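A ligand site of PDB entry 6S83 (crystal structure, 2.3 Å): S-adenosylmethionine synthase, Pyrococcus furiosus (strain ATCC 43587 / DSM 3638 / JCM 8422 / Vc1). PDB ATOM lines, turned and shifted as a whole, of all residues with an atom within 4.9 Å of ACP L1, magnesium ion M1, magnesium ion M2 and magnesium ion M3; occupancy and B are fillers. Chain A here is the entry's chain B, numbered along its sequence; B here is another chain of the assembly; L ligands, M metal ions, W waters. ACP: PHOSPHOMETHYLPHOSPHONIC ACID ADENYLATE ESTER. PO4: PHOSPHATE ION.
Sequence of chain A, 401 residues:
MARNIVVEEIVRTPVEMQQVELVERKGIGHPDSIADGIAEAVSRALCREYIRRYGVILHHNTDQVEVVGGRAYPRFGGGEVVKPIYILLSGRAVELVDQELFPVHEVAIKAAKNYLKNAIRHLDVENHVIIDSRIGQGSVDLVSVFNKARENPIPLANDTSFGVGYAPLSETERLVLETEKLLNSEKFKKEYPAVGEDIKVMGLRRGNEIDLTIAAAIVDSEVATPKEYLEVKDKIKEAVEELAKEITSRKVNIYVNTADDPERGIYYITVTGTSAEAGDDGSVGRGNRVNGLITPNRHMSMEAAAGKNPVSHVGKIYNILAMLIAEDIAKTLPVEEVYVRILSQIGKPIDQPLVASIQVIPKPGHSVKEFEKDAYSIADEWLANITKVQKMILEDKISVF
An oxygen (O3') of ACP L1 lies within hydrogen-bond range of the side-chain hydroxyl (OG) of Ser 275 (2.8 Å). An oxygen (O1B) of ACP L1 sits at hydrogen-bond distance from a ring nitrogen (NE2) of His 313 of chain B (3.3 Å). O3G of ACP L1 lies close to NZ of Lys 26, 3.4 Å away. NE2 of His 30 is in hydrogen-bond range of O2G of ACP L1. OD1 of Asp 198 sits at hydrogen-bond distance from O2' of ACP L1, at 2.8 Å. An oxygen (O2G) of ACP L1 lies within salt-bridge range of the side-chain amino group of Lys 200 (2.7 Å).
NE2 of His 313 of chain B lies close to OE2 of Glu 303 of chain B. The side-chain carboxylate (OD1) of Asp 260 lies within hydrogen-bond range of the backbone NH (N) of Tyr 268, at 3.2 Å. A ring nitrogen (ND1) of His 30 lies within hydrogen-bond range of the backbone NH (N) of Asp 32, at 3.0 Å. The side-chain carboxylate of Asp 32 sits close to the side-chain amino group of Lys 26, 3.2 Å away. The side-chain carboxylate (OD2) of Asp 198 sits at hydrogen-bond distance from the side-chain hydroxyl (OH) of Tyr 268. OD1 of Asp 159 of chain B sits close to OD1 of Asn 158 of chain B (3.1 Å). OD2 of Asp 198 sits at hydrogen-bond distance from OG of Ser 275. O of Lys 200 sits at hydrogen-bond distance from N of Ala 215 (2.8 Å).
OH of Tyr 268 lies close to N9 of ACP L1, at 3.3 Å. Residues that only touch ACP L1: Pro 31 (3.7 Å), Ala 215 (3.6 Å), Ala 259 (3.7 Å), Asp 280 (3.4 Å) and Glu 303 of chain B (3.96 Å). Of the 22 residues printed, 13 come within 4 Å of ACP L1. Along chain A the residues within 4 Å of ACP L1 span positions 26 to 280. The nearest printed residue that does not touch ACP L1 is Asp 159 of chain B (4.4 Å).
The nearest printed residue that does not touch magnesium ion M1 is Asn 158 of chain B (4.1 Å).
NZ of Lys 26 touches magnesium ion M2, at 3.97 Å. Two residues have an atom within 4 Å of magnesium ion M2: Lys 26 and Asp 32. The nearest printed residue that does not touch magnesium ion M2 is His 30 (4.1 Å).
Glu 24 touches magnesium ion M3 (OE2 to MG, 3.6 Å). Of the 22 residues printed, 1 comes within 4 Å of magnesium ion M3. The nearest printed residue that does not touch magnesium ion M3 is Lys 200 (4.2 Å).
Magnesium ion M1 is bound by the side-chain carboxylate (OD2) of Asp 159 of chain B (2.1 Å). Magnesium ion M1 is bound by water W6 (2.2 Å). Water W12 is bound to magnesium ion M1 (2.2 Å). Magnesium ion M1 is bound by water W8 (2.2 Å). Magnesium ion M1 is bound by O2A of ACP L1 (2.3 Å).
Magnesium ion M2 is bound by an oxygen (O3G) of ACP L1 (2.0 Å), an oxygen (O1) of PO4 L2 (2.0 Å), the side-chain carboxylate of Asp 32 (2.1 Å), water W4 (2.1 Å), water W10 (2.1 Å) and water W7 (2.2 Å).
Magnesium ion M3 is bound by O2B of ACP L1 (2.1 Å), water W9 (2.2 Å), water W2 (2.2 Å), water W3 (2.2 Å), O1G of ACP L1 (2.2 Å) and water W11 (2.2 Å). Magnesium ion M3 has six donor atoms within binding distance.
Water W7 lies within hydrogen-bond range of the side-chain carboxylate (OD1) of Asp 32 (2.5 Å), the side-chain amide oxygen (OE1) of Gln 64 of chain B (2.7 Å) and the guanidinium group (NH2) of Arg 286 (3.1 Å). Water W10 bridges the backbone carbonyl oxygen (O) of Asp 281 (2.7 Å) and the side-chain carboxylate (OD1) of Asp 32 (3.4 Å). Water W5 lies within hydrogen-bond range of an oxygen (O3') of ACP L1 and a ring nitrogen (NE2) of His 30. Water W1 lies within hydrogen-bond range of N1 of ACP L1 (2.8 Å), N of Ala 259 (2.9 Å) and OD1 of Asp 260 (3.1 Å).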
ATOM      1  N   GLU A  24     -17.456 -17.010  -6.788  1.00  0.00           N
ATOM      2  CA  GLU A  24     -18.637 -16.241  -7.149  1.00  0.00           C
ATOM      3  C   GLU A  24     -18.786 -15.079  -6.183  1.00  0.00           C
ATOM      4  O   GLU A  24     -18.424 -15.170  -5.011  1.00  0.00           O
ATOM      5  CB  GLU A  24     -19.898 -17.114  -7.130  1.00  0.00           C
ATOM      6  CG  GLU A  24     -21.154 -16.409  -7.624  1.00  0.00           C
ATOM      7  CD  GLU A  24     -22.365 -17.309  -7.635  1.00  0.00           C
ATOM      8  OE1 GLU A  24     -22.328 -18.380  -6.990  1.00  0.00           O
ATOM      9  OE2 GLU A  24     -23.363 -16.949  -8.306  1.00  0.00           O
ATOM     10  N   LYS A  26     -21.832 -11.947  -5.340  1.00  0.00           N
ATOM     11  CA  LYS A  26     -23.119 -11.310  -5.582  1.00  0.00           C
ATOM     12  C   LYS A  26     -22.959  -9.824  -5.281  1.00  0.00           C
ATOM     13  O   LYS A  26     -22.706  -9.436  -4.136  1.00  0.00           O
ATOM     14  CB  LYS A  26     -24.195 -11.950  -4.724  1.00  0.00           C
ATOM     15  CG  LYS A  26     -24.640 -13.331  -5.213  1.00  0.00           C
ATOM     16  CD  LYS A  26     -25.176 -14.183  -4.083  1.00  0.00           C
ATOM     17  CE  LYS A  26     -26.170 -15.228  -4.575  1.00  0.00           C
ATOM     18  NZ  LYS A  26     -26.503 -16.238  -3.532  1.00  0.00           N
ATOM     19  N   HIS A  30     -27.609  -7.209  -5.982  1.00  0.00           N
ATOM     20  CA  HIS A  30     -28.220  -8.532  -5.977  1.00  0.00           C
ATOM     21  C   HIS A  30     -29.178  -8.640  -4.804  1.00  0.00           C
ATOM     22  O   HIS A  30     -28.864  -8.205  -3.689  1.00  0.00           O
ATOM     23  CB  HIS A  30     -27.152  -9.618  -5.885  1.00  0.00           C
ATOM     24  CG  HIS A  30     -27.694 -11.006  -6.017  1.00  0.00           C
ATOM     25  ND1 HIS A  30     -28.299 -11.660  -4.971  1.00  0.00           N
ATOM     26  CD2 HIS A  30     -27.738 -11.850  -7.068  1.00  0.00           C
ATOM     27  CE1 HIS A  30     -28.691 -12.863  -5.365  1.00  0.00           C
ATOM     28  NE2 HIS A  30     -28.354 -13.002  -6.643  1.00  0.00           N
ATOM     29  N   PRO A  31     -30.370  -9.230  -5.004  1.00  0.00           N
ATOM     30  CA  PRO A  31     -31.358  -9.257  -3.900  1.00  0.00           C
ATOM     31  C   PRO A  31     -30.794  -9.788  -2.596  1.00  0.00           C
ATOM     32  O   PRO A  31     -31.040  -9.193  -1.538  1.00  0.00           O
ATOM     33  CB  PRO A  31     -32.465 -10.154  -4.469  1.00  0.00           C
ATOM     34  CG  PRO A  31     -32.363 -10.003  -5.943  1.00  0.00           C
ATOM     35  CD  PRO A  31     -30.898  -9.849  -6.231  1.00  0.00           C
ATOM     36  N   ASP A  32     -30.059 -10.901  -2.627  1.00  0.00           N
ATOM     37  CA  ASP A  32     -29.436 -11.413  -1.414  1.00  0.00           C
ATOM     38  C   ASP A  32     -28.514 -10.381  -0.787  1.00  0.00           C
ATOM     39  O   ASP A  32     -28.523 -10.181   0.425  1.00  0.00           O
ATOM     40  CB  ASP A  32     -28.674 -12.704  -1.719  1.00  0.00           C
ATOM     41  CG  ASP A  32     -29.582 -13.854  -2.079  1.00  0.00           C
ATOM     42  OD1 ASP A  32     -30.691 -13.943  -1.512  1.00  0.00           O
ATOM     43  OD2 ASP A  32     -29.190 -14.674  -2.929  1.00  0.00           O
ATOM     44  N   ASP A 198     -26.996  -4.633  -9.633  1.00  0.00           N
ATOM     45  CA  ASP A 198     -27.186  -6.072  -9.521  1.00  0.00           C
ATOM     46  C   ASP A 198     -26.187  -6.748 -10.453  1.00  0.00           C
ATOM     47  O   ASP A 198     -26.478  -7.044 -11.610  1.00  0.00           O
ATOM     48  CB  ASP A 198     -28.618  -6.464  -9.830  1.00  0.00           C
ATOM     49  CG  ASP A 198     -28.881  -7.945  -9.645  1.00  0.00           C
ATOM     50  OD1 ASP A 198     -27.913  -8.704  -9.387  1.00  0.00           O
ATOM     51  OD2 ASP A 198     -30.052  -8.351  -9.758  1.00  0.00           O
ATOM     52  N   LYS A 200     -23.537  -9.939 -10.797  1.00  0.00           N
ATOM     53  CA  LYS A 200     -23.124 -11.259 -10.346  1.00  0.00           C
ATOM     54  C   LYS A 200     -21.894 -11.673 -11.144  1.00  0.00           C
ATOM     55  O   LYS A 200     -21.926 -11.663 -12.374  1.00  0.00           O
ATOM     56  CB  LYS A 200     -24.245 -12.279 -10.544  1.00  0.00           C
ATOM     57  CG  LYS A 200     -23.917 -13.654  -9.991  1.00  0.00           C
ATOM     58  CD  LYS A 200     -25.048 -14.637 -10.219  1.00  0.00           C
ATOM     59  CE  LYS A 200     -26.226 -14.402  -9.290  1.00  0.00           C
ATOM     60  NZ  LYS A 200     -27.353 -15.306  -9.640  1.00  0.00           N
ATOM     61  N   ALA A 215     -23.034 -11.139 -14.873  1.00  0.00           N
ATOM     62  CA  ALA A 215     -24.435 -10.813 -15.080  1.00  0.00           C
ATOM     63  C   ALA A 215     -24.670  -9.434 -14.474  1.00  0.00           C
ATOM     64  O   ALA A 215     -24.709  -9.303 -13.250  1.00  0.00           O
ATOM     65  CB  ALA A 215     -25.352 -11.870 -14.459  1.00  0.00           C
ATOM     66  N   ALA A 259     -27.290 -14.850 -20.696  1.00  0.00           N
ATOM     67  CA  ALA A 259     -28.659 -15.248 -21.009  1.00  0.00           C
ATOM     68  C   ALA A 259     -29.261 -14.422 -22.148  1.00  0.00           C
ATOM     69  O   ALA A 259     -30.363 -14.744 -22.594  1.00  0.00           O
ATOM     70  CB  ALA A 259     -29.544 -15.124 -19.768  1.00  0.00           C
ATOM     71  N   ASP A 260     -28.576 -13.376 -22.607  1.00  0.00           N
ATOM     72  CA  ASP A 260     -29.112 -12.537 -23.661  1.00  0.00           C
ATOM     73  C   ASP A 260     -29.298 -13.336 -24.943  1.00  0.00           C
ATOM     74  O   ASP A 260     -28.528 -14.230 -25.275  1.00  0.00           O
ATOM     75  CB  ASP A 260     -28.188 -11.354 -23.929  1.00  0.00           C
ATOM     76  CG  ASP A 260     -28.186 -10.340 -22.794  1.00  0.00           C
ATOM     77  OD1 ASP A 260     -28.969 -10.517 -21.847  1.00  0.00           O
ATOM     78  OD2 ASP A 260     -27.394  -9.378 -22.864  1.00  0.00           O
ATOM     79  N   TYR A 267     -33.068  -9.359 -23.315  1.00  0.00           N
ATOM     80  CA  TYR A 267     -31.986  -8.503 -22.842  1.00  0.00           C
ATOM     81  C   TYR A 267     -32.102  -8.333 -21.332  1.00  0.00           C
ATOM     82  O   TYR A 267     -33.207  -8.253 -20.798  1.00  0.00           O
ATOM     83  CB  TYR A 267     -32.026  -7.132 -23.521  1.00  0.00           C
ATOM     84  CG  TYR A 267     -31.836  -7.166 -25.023  1.00  0.00           C
ATOM     85  CD1 TYR A 267     -30.812  -7.900 -25.597  1.00  0.00           C
ATOM     86  CD2 TYR A 267     -32.711  -6.498 -25.856  1.00  0.00           C
ATOM     87  CE1 TYR A 267     -30.636  -7.943 -26.966  1.00  0.00           C
ATOM     88  CE2 TYR A 267     -32.549  -6.521 -27.228  1.00  0.00           C
ATOM     89  CZ  TYR A 267     -31.520  -7.252 -27.780  1.00  0.00           C
ATOM     90  OH  TYR A 267     -31.362  -7.287 -29.146  1.00  0.00           O
ATOM     91  N   TYR A 268     -30.961  -8.279 -20.666  1.00  0.00           N
ATOM     92  CA  TYR A 268     -30.941  -8.081 -19.215  1.00  0.00           C
ATOM     93  C   TYR A 268     -30.951  -6.581 -18.904  1.00  0.00           C
ATOM     94  O   TYR A 268     -29.986  -6.000 -18.395  1.00  0.00           O
ATOM     95  CB  TYR A 268     -29.722  -8.768 -18.599  1.00  0.00           C
ATOM     96  CG  TYR A 268     -29.710  -8.759 -17.080  1.00  0.00           C
ATOM     97  CD1 TYR A 268     -30.837  -8.415 -16.339  1.00  0.00           C
ATOM     98  CD2 TYR A 268     -28.555  -9.082 -16.373  1.00  0.00           C
ATOM     99  CE1 TYR A 268     -30.829  -8.408 -14.967  1.00  0.00           C
ATOM    100  CE2 TYR A 268     -28.533  -9.070 -15.000  1.00  0.00           C
ATOM    101  CZ  TYR A 268     -29.670  -8.735 -14.292  1.00  0.00           C
ATOM    102  OH  TYR A 268     -29.648  -8.723 -12.919  1.00  0.00           O
ATOM    103  N   SER A 275     -32.563  -6.800 -10.148  1.00  0.00           N
ATOM    104  CA  SER A 275     -33.550  -7.802 -10.523  1.00  0.00           C
ATOM    105  C   SER A 275     -34.569  -8.044  -9.420  1.00  0.00           C
ATOM    106  O   SER A 275     -35.526  -8.791  -9.645  1.00  0.00           O
ATOM    107  CB  SER A 275     -32.852  -9.113 -10.884  1.00  0.00           C
ATOM    108  OG  SER A 275     -32.230  -9.693  -9.755  1.00  0.00           O
ATOM    109  N   ASP A 280     -37.439 -11.501  -8.321  1.00  0.00           N
ATOM    110  CA  ASP A 280     -36.285 -12.185  -7.765  1.00  0.00           C
ATOM    111  C   ASP A 280     -36.152 -11.793  -6.301  1.00  0.00           C
ATOM    112  O   ASP A 280     -36.230 -10.604  -5.957  1.00  0.00           O
ATOM    113  CB  ASP A 280     -35.003 -11.861  -8.528  1.00  0.00           C
ATOM    114  CG  ASP A 280     -34.909 -12.592  -9.852  1.00  0.00           C
ATOM    115  OD1 ASP A 280     -35.410 -13.741  -9.923  1.00  0.00           O
ATOM    116  OD2 ASP A 280     -34.331 -12.033 -10.801  1.00  0.00           O
ATOM    117  N   ASP A 281     -35.954 -12.784  -5.449  1.00  0.00           N
ATOM    118  CA  ASP A 281     -36.028 -12.615  -4.015  1.00  0.00           C
ATOM    119  C   ASP A 281     -34.640 -12.638  -3.391  1.00  0.00           C
ATOM    120  O   ASP A 281     -33.680 -13.140  -3.975  1.00  0.00           O
ATOM    121  CB  ASP A 281     -36.895 -13.708  -3.396  1.00  0.00           C
ATOM    122  CG  ASP A 281     -38.237 -13.849  -4.092  1.00  0.00           C
ATOM    123  OD1 ASP A 281     -38.981 -12.843  -4.157  1.00  0.00           O
ATOM    124  OD2 ASP A 281     -38.545 -14.954  -4.575  1.00  0.00           O
ATOM    125  N   ARG A 286     -27.328 -15.366   2.296  1.00  0.00           N
ATOM    126  CA  ARG A 286     -27.479 -16.197   1.107  1.00  0.00           C
ATOM    127  C   ARG A 286     -26.438 -15.897   0.042  1.00  0.00           C
ATOM    128  O   ARG A 286     -26.507 -16.460  -1.058  1.00  0.00           O
ATOM    129  CB  ARG A 286     -28.887 -16.016   0.532  1.00  0.00           C
ATOM    130  CG  ARG A 286     -29.976 -16.597   1.408  1.00  0.00           C
ATOM    131  CD  ARG A 286     -30.042 -18.109   1.274  1.00  0.00           C
ATOM    132  NE  ARG A 286     -30.638 -18.518  -0.001  1.00  0.00           N
ATOM    133  CZ  ARG A 286     -31.943 -18.692  -0.206  1.00  0.00           C
ATOM    134  NH1 ARG A 286     -32.809 -18.504   0.782  1.00  0.00           N
ATOM    135  NH2 ARG A 286     -32.372 -19.057  -1.400  1.00  0.00           N
ATOM    136  N   GLN B  64     -37.554 -19.196   0.049  1.00  0.00           N
ATOM    137  CA  GLN B  64     -37.604 -17.890   0.700  1.00  0.00           C
ATOM    138  C   GLN B  64     -38.694 -17.981   1.767  1.00  0.00           C
ATOM    139  O   GLN B  64     -39.878 -17.830   1.468  1.00  0.00           O
ATOM    140  CB  GLN B  64     -37.898 -16.783  -0.302  1.00  0.00           C
ATOM    141  CG  GLN B  64     -36.904 -16.700  -1.452  1.00  0.00           C
ATOM    142  CD  GLN B  64     -35.495 -16.307  -1.027  1.00  0.00           C
ATOM    143  OE1 GLN B  64     -34.523 -16.651  -1.699  1.00  0.00           O
ATOM    144  NE2 GLN B  64     -35.367 -15.563   0.064  1.00  0.00           N
ATOM    145  N   ASN B 158     -28.917 -23.917 -18.265  1.00  0.00           N
ATOM    146  CA  ASN B 158     -28.853 -22.542 -18.737  1.00  0.00           C
ATOM    147  C   ASN B 158     -27.732 -21.745 -18.084  1.00  0.00           C
ATOM    148  O   ASN B 158     -27.456 -20.627 -18.517  1.00  0.00           O
ATOM    149  CB  ASN B 158     -30.190 -21.836 -18.485  1.00  0.00           C
ATOM    150  CG  ASN B 158     -30.595 -21.841 -17.029  1.00  0.00           C
ATOM    151  OD1 ASN B 158     -29.840 -22.298 -16.159  1.00  0.00           O
ATOM    152  ND2 ASN B 158     -31.797 -21.342 -16.740  1.00  0.00           N
ATOM    153  N   ASP B 159     -27.069 -22.313 -17.068  1.00  0.00           N
ATOM    154  CA  ASP B 159     -26.016 -21.617 -16.349  1.00  0.00           C
ATOM    155  C   ASP B 159     -24.970 -22.636 -15.923  1.00  0.00           C
ATOM    156  O   ASP B 159     -25.145 -23.845 -16.076  1.00  0.00           O
ATOM    157  CB  ASP B 159     -26.574 -20.865 -15.127  1.00  0.00           C
ATOM    158  CG  ASP B 159     -27.300 -21.783 -14.157  1.00  0.00           C
ATOM    159  OD1 ASP B 159     -27.357 -23.013 -14.405  1.00  0.00           O
ATOM    160  OD2 ASP B 159     -27.823 -21.269 -13.135  1.00  0.00           O
ATOM    161  N   GLU B 303     -25.259 -22.513  -1.733  1.00  0.00           N
ATOM    162  CA  GLU B 303     -26.603 -22.567  -2.288  1.00  0.00           C
ATOM    163  C   GLU B 303     -27.554 -23.246  -1.310  1.00  0.00           C
ATOM    164  O   GLU B 303     -27.283 -24.337  -0.805  1.00  0.00           O
ATOM    165  CB  GLU B 303     -26.581 -23.332  -3.609  1.00  0.00           C
ATOM    166  CG  GLU B 303     -27.690 -22.940  -4.559  1.00  0.00           C
ATOM    167  CD  GLU B 303     -27.468 -23.486  -5.947  1.00  0.00           C
ATOM    168  OE1 GLU B 303     -26.955 -24.612  -6.067  1.00  0.00           O
ATOM    169  OE2 GLU B 303     -27.794 -22.776  -6.922  1.00  0.00           O
ATOM    170  N   LYS B 308     -36.137 -25.236  -3.390  1.00  0.00           N
ATOM    171  CA  LYS B 308     -35.849 -25.157  -4.819  1.00  0.00           C
ATOM    172  C   LYS B 308     -36.485 -26.323  -5.560  1.00  0.00           C
ATOM    173  O   LYS B 308     -36.598 -27.430  -5.046  1.00  0.00           O
ATOM    174  CB  LYS B 308     -34.335 -25.111  -5.058  1.00  0.00           C
ATOM    175  CG  LYS B 308     -33.719 -23.808  -4.599  1.00  0.00           C
ATOM    176  CD  LYS B 308     -32.250 -23.714  -4.968  1.00  0.00           C
ATOM    177  CE  LYS B 308     -31.798 -22.254  -4.968  1.00  0.00           C
ATOM    178  NZ  LYS B 308     -31.587 -21.703  -3.594  1.00  0.00           N
ATOM    179  N   HIS B 313     -34.163 -27.066 -10.921  1.00  0.00           N
ATOM    180  CA  HIS B 313     -33.025 -26.372 -10.342  1.00  0.00           C
ATOM    181  C   HIS B 313     -31.831 -27.324 -10.329  1.00  0.00           C
ATOM    182  O   HIS B 313     -31.815 -28.309  -9.584  1.00  0.00           O
ATOM    183  CB  HIS B 313     -33.318 -25.839  -8.945  1.00  0.00           C
ATOM    184  CG  HIS B 313     -32.296 -24.848  -8.471  1.00  0.00           C
ATOM    185  ND1 HIS B 313     -31.040 -25.233  -8.047  1.00  0.00           N
ATOM    186  CD2 HIS B 313     -32.319 -23.497  -8.424  1.00  0.00           C
ATOM    187  CE1 HIS B 313     -30.343 -24.163  -7.725  1.00  0.00           C
ATOM    188  NE2 HIS B 313     -31.092 -23.089  -7.935  1.00  0.00           N
HETATM  189  PG  ACP L   1     -29.068 -16.512  -6.694  1.00  0.00           P
HETATM  190  O1G ACP L   1     -27.665 -17.082  -6.729  1.00  0.00           O
HETATM  191  O2G ACP L   1     -29.160 -15.330  -7.628  1.00  0.00           O
HETATM  192  O3G ACP L   1     -29.381 -16.052  -5.287  1.00  0.00           O
HETATM  193  PB  ACP L   1     -29.623 -18.743  -8.661  1.00  0.00           P
HETATM  194  O1B ACP L   1     -30.430 -19.996  -8.879  1.00  0.00           O
HETATM  195  O2B ACP L   1     -28.174 -19.115  -8.377  1.00  0.00           O
HETATM  196  C3B ACP L   1     -30.290 -17.808  -7.202  1.00  0.00           C
HETATM  197  PA  ACP L   1     -31.038 -17.508 -10.881  1.00  0.00           P
HETATM  198  O1A ACP L   1     -32.245 -17.660 -10.006  1.00  0.00           O
HETATM  199  O2A ACP L   1     -31.080 -18.518 -12.003  1.00  0.00           O
HETATM  200  O3A ACP L   1     -29.677 -17.770  -9.984  1.00  0.00           O
HETATM  201  O5' ACP L   1     -30.977 -15.984 -11.507  1.00  0.00           O
HETATM  202  C5' ACP L   1     -31.466 -14.905 -10.742  1.00  0.00           C
HETATM  203  C4' ACP L   1     -30.363 -13.815 -10.638  1.00  0.00           C
HETATM  204  O4' ACP L   1     -29.708 -13.729 -11.764  1.00  0.00           O
HETATM  205  C3' ACP L   1     -30.982 -12.423 -10.411  1.00  0.00           C
HETATM  206  O3' ACP L   1     -31.043 -12.139  -9.078  1.00  0.00           O
HETATM  207  C2' ACP L   1     -29.989 -11.483 -11.122  1.00  0.00           C
HETATM  208  O2' ACP L   1     -28.811 -11.205 -10.253  1.00  0.00           O
HETATM  209  C1' ACP L   1     -29.602 -12.164 -12.170  1.00  0.00           C
HETATM  210  N9  ACP L   1     -30.420 -11.923 -13.344  1.00  0.00           N
HETATM  211  C8  ACP L   1     -31.693 -11.513 -13.424  1.00  0.00           C
HETATM  212  N7  ACP L   1     -32.023 -11.448 -14.722  1.00  0.00           N
HETATM  213  C5  ACP L   1     -30.966 -11.833 -15.441  1.00  0.00           C
HETATM  214  C6  ACP L   1     -30.765 -11.948 -16.801  1.00  0.00           C
HETATM  215  N6  ACP L   1     -31.623 -11.709 -17.943  1.00  0.00           N
HETATM  216  N1  ACP L   1     -29.598 -12.356 -17.270  1.00  0.00           N
HETATM  217  C2  ACP L   1     -28.595 -12.659 -16.405  1.00  0.00           C
HETATM  218  N3  ACP L   1     -28.787 -12.539 -15.075  1.00  0.00           N
HETATM  219  C4  ACP L   1     -29.973 -12.126 -14.593  1.00  0.00           C
HETATM  220  P   PO4 L   2     -28.988 -18.910  -3.107  1.00  0.00           P
HETATM  221  O1  PO4 L   2     -29.621 -17.654  -2.545  1.00  0.00           O
HETATM  222  O2  PO4 L   2     -28.675 -19.855  -1.974  1.00  0.00           O
HETATM  223  O3  PO4 L   2     -29.946 -19.573  -4.070  1.00  0.00           O
HETATM  224  O4  PO4 L   2     -27.714 -18.548  -3.827  1.00  0.00           O
HETATM  225 MG    MG M   1     -29.593 -20.186 -12.711  1.00  0.00          MG
HETATM  226 MG    MG M   2     -30.468 -16.143  -3.624  1.00  0.00          MG
HETATM  227 MG    MG M   3     -26.383 -18.742  -7.427  1.00  0.00          MG
HETATM  228  O   HOH W   1     -27.978 -12.238 -19.520  1.00  0.00           O
HETATM  229  O   HOH W   2     -27.415 -19.898  -5.933  1.00  0.00           O
HETATM  230  O   HOH W   3     -24.841 -18.131  -5.978  1.00  0.00           O
HETATM  231  O   HOH W   4     -31.538 -17.743  -4.387  1.00  0.00           O
HETATM  232  O   HOH W   5     -31.555 -14.030  -7.146  1.00  0.00           O
HETATM  233  O   HOH W   6     -30.004 -21.452 -11.001  1.00  0.00           O
HETATM  234  O   HOH W   7     -31.897 -16.052  -1.914  1.00  0.00           O
HETATM  235  O   HOH W   8     -31.017 -19.553 -14.308  1.00  0.00           O
HETATM  236  O   HOH W   9     -25.441 -17.591  -8.982  1.00  0.00           O
HETATM  237  O   HOH W  10     -31.687 -14.756  -4.664  1.00  0.00           O
HETATM  238  O   HOH W  11     -26.055 -20.578  -8.615  1.00  0.00           O
HETATM  239  O   HOH W  12     -28.609 -18.349 -13.389  1.00  0.00           O
